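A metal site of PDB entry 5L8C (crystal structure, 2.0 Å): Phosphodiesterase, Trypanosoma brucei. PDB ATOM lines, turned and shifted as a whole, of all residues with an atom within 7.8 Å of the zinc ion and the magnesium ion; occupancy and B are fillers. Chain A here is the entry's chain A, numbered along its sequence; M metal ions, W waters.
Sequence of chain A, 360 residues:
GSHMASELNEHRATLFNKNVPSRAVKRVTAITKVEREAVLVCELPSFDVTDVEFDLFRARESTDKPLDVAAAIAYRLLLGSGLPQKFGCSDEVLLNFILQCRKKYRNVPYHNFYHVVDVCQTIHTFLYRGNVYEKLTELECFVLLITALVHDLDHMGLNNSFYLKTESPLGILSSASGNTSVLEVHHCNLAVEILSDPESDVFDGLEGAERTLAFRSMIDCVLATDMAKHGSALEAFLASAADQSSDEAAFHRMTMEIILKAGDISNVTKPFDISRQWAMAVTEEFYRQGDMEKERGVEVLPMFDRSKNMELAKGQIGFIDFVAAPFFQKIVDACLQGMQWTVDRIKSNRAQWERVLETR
Within 4 Å of the zinc ion: His 115, His 151, Asp 152 and Asp 264. Along chain A the residues within 4 Å of the zinc ion span positions 115 to 264.
The zinc ion is bound by OD2 of Asp 152 (2.0 Å), OD1 of Asp 264 (2.1 Å), NE2 of His 115 (2.3 Å), water W4 (2.3 Å), NE2 of His 151 (2.3 Å) and water W2 (2.3 Å).
Water W1 lies within hydrogen-bond range of the side-chain hydroxyl (OG1) of Thr 225 (2.5 Å) and the backbone carbonyl oxygen (O) of His 151 (2.7 Å). Water W6 bridges a ring nitrogen (NE2) of His 187 and the side-chain carboxylate of Glu 184. Water W5 bridges the side-chain carboxylate of Glu 184 (2.8 Å) and the backbone carbonyl oxygen of Thr 225 (2.9 Å). Water W3 lies within hydrogen-bond range of NE2 of His 111 (2.9 Å) and NE2 of His 155 (3.4 Å).
Merely in contact with the magnesium ion: Thr 225 (3.96 Å). Within 4 Å of the magnesium ion: Asp 152 and Thr 225.
The magnesium ion is bound by water W4 (1.8 Å), water W6 (1.8 Å), water W1 (2.0 Å), OD1 of Asp 152 (2.0 Å), water W5 (2.2 Å) and water W3 (2.2 Å). The magnesium ion has six donor atoms within binding distance.
The backbone NH (N) of Asp 152 sits at hydrogen-bond distance from the side-chain hydroxyl (OH) of Tyr 105. The side-chain hydroxyl (OG1) of Thr 225 sits at hydrogen-bond distance from the backbone carbonyl oxygen (O) of Val 222. ND1 of His 151 sits at hydrogen-bond distance from O of Ala 148 (2.7 Å). The backbone NH of His 115 lies within hydrogen-bond range of the side-chain amide oxygen of Asn 112 (3.3 Å).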
ATOM      1  N   TYR A 105       8.041  12.094 -17.934  1.00  0.00           N
ATOM      2  CA  TYR A 105       7.684  12.865 -19.137  1.00  0.00           C
ATOM      3  C   TYR A 105       8.940  13.036 -19.909  1.00  0.00           C
ATOM      4  O   TYR A 105      10.037  13.034 -19.347  1.00  0.00           O
ATOM      5  CB  TYR A 105       6.974  14.222 -18.857  1.00  0.00           C
ATOM      6  CG  TYR A 105       5.538  14.008 -18.419  1.00  0.00           C
ATOM      7  CD1 TYR A 105       4.534  13.878 -19.354  1.00  0.00           C
ATOM      8  CD2 TYR A 105       5.224  13.855 -17.085  1.00  0.00           C
ATOM      9  CE1 TYR A 105       3.224  13.621 -18.939  1.00  0.00           C
ATOM     10  CE2 TYR A 105       3.926  13.593 -16.662  1.00  0.00           C
ATOM     11  CZ  TYR A 105       2.932  13.465 -17.598  1.00  0.00           C
ATOM     12  OH  TYR A 105       1.643  13.200 -17.204  1.00  0.00           O
ATOM     13  N   TYR A 110       5.421  19.169 -27.246  1.00  0.00           N
ATOM     14  CA  TYR A 110       4.146  19.504 -26.636  1.00  0.00           C
ATOM     15  C   TYR A 110       3.786  18.649 -25.449  1.00  0.00           C
ATOM     16  O   TYR A 110       3.588  19.155 -24.386  1.00  0.00           O
ATOM     17  CB  TYR A 110       3.017  19.515 -27.652  1.00  0.00           C
ATOM     18  CG  TYR A 110       1.685  19.938 -27.107  1.00  0.00           C
ATOM     19  CD1 TYR A 110       1.360  21.261 -26.944  1.00  0.00           C
ATOM     20  CD2 TYR A 110       0.743  19.004 -26.772  1.00  0.00           C
ATOM     21  CE1 TYR A 110       0.143  21.640 -26.458  1.00  0.00           C
ATOM     22  CE2 TYR A 110      -0.483  19.374 -26.291  1.00  0.00           C
ATOM     23  CZ  TYR A 110      -0.768  20.697 -26.121  1.00  0.00           C
ATOM     24  OH  TYR A 110      -1.971  21.048 -25.644  1.00  0.00           O
ATOM     25  N   HIS A 111       3.713  17.351 -25.624  1.00  0.00           N
ATOM     26  CA  HIS A 111       3.350  16.495 -24.523  1.00  0.00           C
ATOM     27  C   HIS A 111       4.461  16.244 -23.535  1.00  0.00           C
ATOM     28  O   HIS A 111       4.872  15.143 -23.338  1.00  0.00           O
ATOM     29  CB  HIS A 111       2.776  15.201 -25.027  1.00  0.00           C
ATOM     30  CG  HIS A 111       1.524  15.373 -25.804  1.00  0.00           C
ATOM     31  ND1 HIS A 111       1.502  15.384 -27.164  1.00  0.00           N
ATOM     32  CD2 HIS A 111       0.247  15.511 -25.403  1.00  0.00           C
ATOM     33  CE1 HIS A 111       0.268  15.537 -27.578  1.00  0.00           C
ATOM     34  NE2 HIS A 111      -0.515  15.609 -26.535  1.00  0.00           N
ATOM     35  N   ASN A 112       4.933  17.297 -22.914  1.00  0.00           N
ATOM     36  CA  ASN A 112       5.964  17.183 -21.942  1.00  0.00           C
ATOM     37  C   ASN A 112       5.361  17.495 -20.600  1.00  0.00           C
ATOM     38  O   ASN A 112       4.177  17.540 -20.472  1.00  0.00           O
ATOM     39  CB  ASN A 112       7.096  18.133 -22.270  1.00  0.00           C
ATOM     40  CG  ASN A 112       6.628  19.520 -22.604  1.00  0.00           C
ATOM     41  OD1 ASN A 112       5.886  20.118 -21.864  1.00  0.00           O
ATOM     42  ND2 ASN A 112       7.099  20.052 -23.699  1.00  0.00           N
ATOM     43  N   HIS A 115       3.026  20.669 -20.265  1.00  0.00           N
ATOM     44  CA  HIS A 115       1.631  20.475 -20.650  1.00  0.00           C
ATOM     45  C   HIS A 115       0.762  19.978 -19.510  1.00  0.00           C
ATOM     46  O   HIS A 115      -0.387  20.422 -19.332  1.00  0.00           O
ATOM     47  CB  HIS A 115       1.538  19.503 -21.796  1.00  0.00           C
ATOM     48  CG  HIS A 115       0.169  18.968 -22.041  1.00  0.00           C
ATOM     49  ND1 HIS A 115      -0.874  19.748 -22.478  1.00  0.00           N
ATOM     50  CD2 HIS A 115      -0.313  17.711 -21.958  1.00  0.00           C
ATOM     51  CE1 HIS A 115      -1.944  18.977 -22.672  1.00  0.00           C
ATOM     52  NE2 HIS A 115      -1.609  17.740 -22.363  1.00  0.00           N
ATOM     53  N   VAL A 116       1.264  19.052 -18.728  1.00  0.00           N
ATOM     54  CA  VAL A 116       0.386  18.442 -17.726  1.00  0.00           C
ATOM     55  C   VAL A 116       0.280  19.400 -16.524  1.00  0.00           C
ATOM     56  O   VAL A 116      -0.736  19.418 -15.876  1.00  0.00           O
ATOM     57  CB  VAL A 116       0.785  16.985 -17.357  1.00  0.00           C
ATOM     58  CG1 VAL A 116       0.932  16.140 -18.609  1.00  0.00           C
ATOM     59  CG2 VAL A 116       2.057  16.904 -16.532  1.00  0.00           C
ATOM     60  N   VAL A 119      -2.329  21.781 -17.650  1.00  0.00           N
ATOM     61  CA  VAL A 119      -3.675  21.202 -17.500  1.00  0.00           C
ATOM     62  C   VAL A 119      -4.122  21.175 -16.036  1.00  0.00           C
ATOM     63  O   VAL A 119      -5.259  21.509 -15.715  1.00  0.00           O
ATOM     64  CB  VAL A 119      -3.710  19.791 -18.101  1.00  0.00           C
ATOM     65  CG1 VAL A 119      -5.051  19.092 -17.779  1.00  0.00           C
ATOM     66  CG2 VAL A 119      -3.484  19.861 -19.627  1.00  0.00           C
ATOM     67  N   ALA A 148      -4.547  15.278 -13.619  1.00  0.00           N
ATOM     68  CA  ALA A 148      -3.927  16.143 -14.605  1.00  0.00           C
ATOM     69  C   ALA A 148      -2.433  15.823 -14.783  1.00  0.00           C
ATOM     70  O   ALA A 148      -1.919  15.851 -15.890  1.00  0.00           O
ATOM     71  CB  ALA A 148      -4.128  17.573 -14.225  1.00  0.00           C
ATOM     72  N   HIS A 151      -1.871  12.299 -16.805  1.00  0.00           N
ATOM     73  CA  HIS A 151      -2.773  11.913 -17.883  1.00  0.00           C
ATOM     74  C   HIS A 151      -2.081  11.738 -19.266  1.00  0.00           C
ATOM     75  O   HIS A 151      -2.696  11.233 -20.198  1.00  0.00           O
ATOM     76  CB  HIS A 151      -3.946  12.927 -17.993  1.00  0.00           C
ATOM     77  CG  HIS A 151      -3.610  14.120 -18.846  1.00  0.00           C
ATOM     78  ND1 HIS A 151      -2.927  15.210 -18.364  1.00  0.00           N
ATOM     79  CD2 HIS A 151      -3.782  14.339 -20.175  1.00  0.00           C
ATOM     80  CE1 HIS A 151      -2.721  16.071 -19.342  1.00  0.00           C
ATOM     81  NE2 HIS A 151      -3.233  15.565 -20.449  1.00  0.00           N
ATOM     82  N   ASP A 152      -0.818  12.135 -19.382  1.00  0.00           N
ATOM     83  CA  ASP A 152      -0.011  11.987 -20.591  1.00  0.00           C
ATOM     84  C   ASP A 152       1.381  11.336 -20.299  1.00  0.00           C
ATOM     85  O   ASP A 152       2.283  11.431 -21.073  1.00  0.00           O
ATOM     86  CB  ASP A 152       0.179  13.313 -21.343  1.00  0.00           C
ATOM     87  CG  ASP A 152      -1.028  13.689 -22.243  1.00  0.00           C
ATOM     88  OD1 ASP A 152      -1.632  12.790 -22.825  1.00  0.00           O
ATOM     89  OD2 ASP A 152      -1.367  14.884 -22.337  1.00  0.00           O
ATOM     90  N   LEU A 153       1.518  10.663 -19.168  1.00  0.00           N
ATOM     91  CA  LEU A 153       2.772  10.013 -18.794  1.00  0.00           C
ATOM     92  C   LEU A 153       3.498   9.210 -19.856  1.00  0.00           C
ATOM     93  O   LEU A 153       2.979   8.291 -20.414  1.00  0.00           O
ATOM     94  CB  LEU A 153       2.572   9.108 -17.579  1.00  0.00           C
ATOM     95  CG  LEU A 153       2.433   9.721 -16.206  1.00  0.00           C
ATOM     96  CD1 LEU A 153       1.929   8.675 -15.240  1.00  0.00           C
ATOM     97  CD2 LEU A 153       3.720  10.334 -15.736  1.00  0.00           C
ATOM     98  N   HIS A 155       4.551  10.092 -22.886  1.00  0.00           N
ATOM     99  CA  HIS A 155       4.157  10.358 -24.284  1.00  0.00           C
ATOM    100  C   HIS A 155       5.451  10.611 -25.079  1.00  0.00           C
ATOM    101  O   HIS A 155       6.415  11.168 -24.564  1.00  0.00           O
ATOM    102  CB  HIS A 155       3.238  11.598 -24.325  1.00  0.00           C
ATOM    103  CG  HIS A 155       2.295  11.676 -25.492  1.00  0.00           C
ATOM    104  ND1 HIS A 155       2.715  11.952 -26.757  1.00  0.00           N
ATOM    105  CD2 HIS A 155       0.944  11.626 -25.552  1.00  0.00           C
ATOM    106  CE1 HIS A 155       1.679  12.014 -27.568  1.00  0.00           C
ATOM    107  NE2 HIS A 155       0.585  11.820 -26.859  1.00  0.00           N
ATOM    108  N   ASN A 160      -2.016   7.905 -31.239  1.00  0.00           N
ATOM    109  CA  ASN A 160      -2.443   6.515 -31.255  1.00  0.00           C
ATOM    110  C   ASN A 160      -2.353   5.955 -32.658  1.00  0.00           C
ATOM    111  O   ASN A 160      -1.867   4.836 -32.876  1.00  0.00           O
ATOM    112  CB  ASN A 160      -3.870   6.347 -30.689  1.00  0.00           C
ATOM    113  CG  ASN A 160      -3.937   6.500 -29.192  1.00  0.00           C
ATOM    114  OD1 ASN A 160      -2.923   6.353 -28.473  1.00  0.00           O
ATOM    115  ND2 ASN A 160      -5.130   6.790 -28.697  1.00  0.00           N
ATOM    116  N   LEU A 183      -2.339   5.046 -26.180  1.00  0.00           N
ATOM    117  CA  LEU A 183      -1.544   5.857 -25.233  1.00  0.00           C
ATOM    118  C   LEU A 183      -2.198   5.971 -23.862  1.00  0.00           C
ATOM    119  O   LEU A 183      -1.542   5.950 -22.821  1.00  0.00           O
ATOM    120  CB  LEU A 183      -1.314   7.251 -25.761  1.00  0.00           C
ATOM    121  CG  LEU A 183      -0.341   7.367 -26.934  1.00  0.00           C
ATOM    122  CD1 LEU A 183      -0.712   8.527 -27.854  1.00  0.00           C
ATOM    123  CD2 LEU A 183       1.087   7.506 -26.432  1.00  0.00           C
ATOM    124  N   GLU A 184      -3.508   6.074 -23.871  1.00  0.00           N
ATOM    125  CA  GLU A 184      -4.241   6.345 -22.649  1.00  0.00           C
ATOM    126  C   GLU A 184      -4.113   5.194 -21.676  1.00  0.00           C
ATOM    127  O   GLU A 184      -3.885   5.390 -20.472  1.00  0.00           O
ATOM    128  CB  GLU A 184      -5.707   6.736 -22.951  1.00  0.00           C
ATOM    129  CG  GLU A 184      -5.815   8.093 -23.688  1.00  0.00           C
ATOM    130  CD  GLU A 184      -5.444   8.082 -25.180  1.00  0.00           C
ATOM    131  OE1 GLU A 184      -5.471   7.018 -25.836  1.00  0.00           O
ATOM    132  OE2 GLU A 184      -5.108   9.171 -25.676  1.00  0.00           O
ATOM    133  N   HIS A 187      -0.713   5.414 -20.240  1.00  0.00           N
ATOM    134  CA  HIS A 187      -0.591   6.431 -19.189  1.00  0.00           C
ATOM    135  C   HIS A 187      -1.139   5.866 -17.885  1.00  0.00           C
ATOM    136  O   HIS A 187      -0.533   6.048 -16.843  1.00  0.00           O
ATOM    137  CB  HIS A 187      -1.269   7.802 -19.516  1.00  0.00           C
ATOM    138  CG  HIS A 187      -0.984   8.353 -20.877  1.00  0.00           C
ATOM    139  ND1 HIS A 187       0.292   8.457 -21.393  1.00  0.00           N
ATOM    140  CD2 HIS A 187      -1.821   8.811 -21.835  1.00  0.00           C
ATOM    141  CE1 HIS A 187       0.216   8.963 -22.611  1.00  0.00           C
ATOM    142  NE2 HIS A 187      -1.053   9.183 -22.900  1.00  0.00           N
ATOM    143  N   VAL A 222      -8.625   9.670 -17.596  1.00  0.00           N
ATOM    144  CA  VAL A 222      -7.526   9.537 -18.555  1.00  0.00           C
ATOM    145  C   VAL A 222      -7.984   8.811 -19.847  1.00  0.00           C
ATOM    146  O   VAL A 222      -7.701   9.251 -20.929  1.00  0.00           O
ATOM    147  CB  VAL A 222      -6.355   8.752 -17.969  1.00  0.00           C
ATOM    148  CG1 VAL A 222      -5.282   8.562 -19.025  1.00  0.00           C
ATOM    149  CG2 VAL A 222      -5.804   9.443 -16.752  1.00  0.00           C
ATOM    150  N   THR A 225      -9.685  11.066 -22.340  1.00  0.00           N
ATOM    151  CA  THR A 225      -8.902  12.069 -23.094  1.00  0.00           C
ATOM    152  C   THR A 225      -8.517  11.634 -24.489  1.00  0.00           C
ATOM    153  O   THR A 225      -7.919  12.442 -25.242  1.00  0.00           O
ATOM    154  CB  THR A 225      -7.602  12.457 -22.390  1.00  0.00           C
ATOM    155  OG1 THR A 225      -6.689  11.334 -22.342  1.00  0.00           O
ATOM    156  CG2 THR A 225      -7.903  12.927 -21.032  1.00  0.00           C
ATOM    157  N   ASP A 226      -8.795  10.365 -24.860  1.00  0.00           N
ATOM    158  CA  ASP A 226      -8.608   9.912 -26.226  1.00  0.00           C
ATOM    159  C   ASP A 226      -9.624  10.652 -27.124  1.00  0.00           C
ATOM    160  O   ASP A 226     -10.835  10.474 -26.962  1.00  0.00           O
ATOM    161  CB  ASP A 226      -8.828   8.406 -26.304  1.00  0.00           C
ATOM    162  CG  ASP A 226      -8.728   7.831 -27.755  1.00  0.00           C
ATOM    163  OD1 ASP A 226      -8.798   8.563 -28.769  1.00  0.00           O
ATOM    164  OD2 ASP A 226      -8.579   6.627 -27.872  1.00  0.00           O
ATOM    165  N   MET A 227      -9.146  11.453 -28.095  1.00  0.00           N
ATOM    166  CA  MET A 227     -10.045  12.325 -28.882  1.00  0.00           C
ATOM    167  C   MET A 227     -10.948  11.565 -29.814  1.00  0.00           C
ATOM    168  O   MET A 227     -11.912  12.136 -30.308  1.00  0.00           O
ATOM    169  CB  MET A 227      -9.299  13.437 -29.641  1.00  0.00           C
ATOM    170  CG  MET A 227      -8.799  14.586 -28.750  1.00  0.00           C
ATOM    171  SD  MET A 227     -10.096  15.499 -27.884  1.00  0.00           S
ATOM    172  CE  MET A 227     -10.842  16.393 -29.252  1.00  0.00           C
ATOM    173  N   LEU A 260     -11.421  17.206 -17.281  1.00  0.00           N
ATOM    174  CA  LEU A 260     -10.079  16.867 -17.769  1.00  0.00           C
ATOM    175  C   LEU A 260      -9.990  17.051 -19.269  1.00  0.00           C
ATOM    176  O   LEU A 260      -8.994  17.568 -19.754  1.00  0.00           O
ATOM    177  CB  LEU A 260      -9.665  15.446 -17.414  1.00  0.00           C
ATOM    178  CG  LEU A 260      -8.254  15.060 -17.859  1.00  0.00           C
ATOM    179  CD1 LEU A 260      -7.182  15.893 -17.195  1.00  0.00           C
ATOM    180  CD2 LEU A 260      -8.039  13.614 -17.517  1.00  0.00           C
ATOM    181  N   LYS A 261     -11.036  16.645 -20.011  1.00  0.00           N
ATOM    182  CA  LYS A 261     -11.035  16.899 -21.450  1.00  0.00           C
ATOM    183  C   LYS A 261     -10.893  18.417 -21.732  1.00  0.00           C
ATOM    184  O   LYS A 261     -10.033  18.858 -22.567  1.00  0.00           O
ATOM    185  CB  LYS A 261     -12.313  16.373 -22.094  1.00  0.00           C
ATOM    186  CG  LYS A 261     -12.314  14.899 -22.376  1.00  0.00           C
ATOM    187  CD  LYS A 261     -13.612  14.435 -23.059  1.00  0.00           C
ATOM    188  CE  LYS A 261     -13.880  15.111 -24.390  1.00  0.00           C
ATOM    189  NZ  LYS A 261     -12.673  15.295 -25.293  1.00  0.00           N
ATOM    190  N   GLY A 263      -9.583  20.854 -19.801  1.00  0.00           N
ATOM    191  CA  GLY A 263      -8.195  21.253 -19.603  1.00  0.00           C
ATOM    192  C   GLY A 263      -7.289  20.851 -20.769  1.00  0.00           C
ATOM    193  O   GLY A 263      -6.370  21.589 -21.127  1.00  0.00           O
ATOM    194  N   ASP A 264      -7.537  19.669 -21.329  1.00  0.00           N
ATOM    195  CA  ASP A 264      -6.697  19.142 -22.363  1.00  0.00           C
ATOM    196  C   ASP A 264      -6.815  19.898 -23.697  1.00  0.00           C
ATOM    197  O   ASP A 264      -5.871  19.923 -24.451  1.00  0.00           O
ATOM    198  CB  ASP A 264      -7.027  17.638 -22.619  1.00  0.00           C
ATOM    199  CG  ASP A 264      -5.801  16.811 -22.975  1.00  0.00           C
ATOM    200  OD1 ASP A 264      -4.703  17.229 -22.624  1.00  0.00           O
ATOM    201  OD2 ASP A 264      -5.931  15.716 -23.552  1.00  0.00           O
ATOM    202  N   ILE A 265      -8.000  20.449 -23.989  1.00  0.00           N
ATOM    203  CA  ILE A 265      -8.170  21.350 -25.118  1.00  0.00           C
ATOM    204  C   ILE A 265      -8.347  22.826 -24.747  1.00  0.00           C
ATOM    205  O   ILE A 265      -8.970  23.618 -25.481  1.00  0.00           O
ATOM    206  CB  ILE A 265      -9.309  20.898 -26.036  1.00  0.00           C
ATOM    207  CG1 ILE A 265     -10.645  20.850 -25.313  1.00  0.00           C
ATOM    208  CG2 ILE A 265      -9.012  19.519 -26.577  1.00  0.00           C
ATOM    209  CD1 ILE A 265     -11.792  20.651 -26.277  1.00  0.00           C
HETATM  210 ZN    ZN M   1      -2.978  15.984 -22.691  1.00  0.00          ZN
HETATM  211 MG    MG M   2      -3.275  12.462 -24.001  1.00  0.00          MG
HETATM  212  O   HOH W   1      -4.158  11.472 -22.514  1.00  0.00           O
HETATM  213  O   HOH W   2      -2.713  16.320 -24.969  1.00  0.00           O
HETATM  214  O   HOH W   3      -2.194  13.413 -25.715  1.00  0.00           O
HETATM  215  O   HOH W   4      -3.872  14.072 -23.539  1.00  0.00           O
HETATM  216  O   HOH W   5      -5.139  11.860 -24.894  1.00  0.00           O
HETATM  217  O   HOH W   6      -2.721  10.861 -24.708  1.00  0.00           O
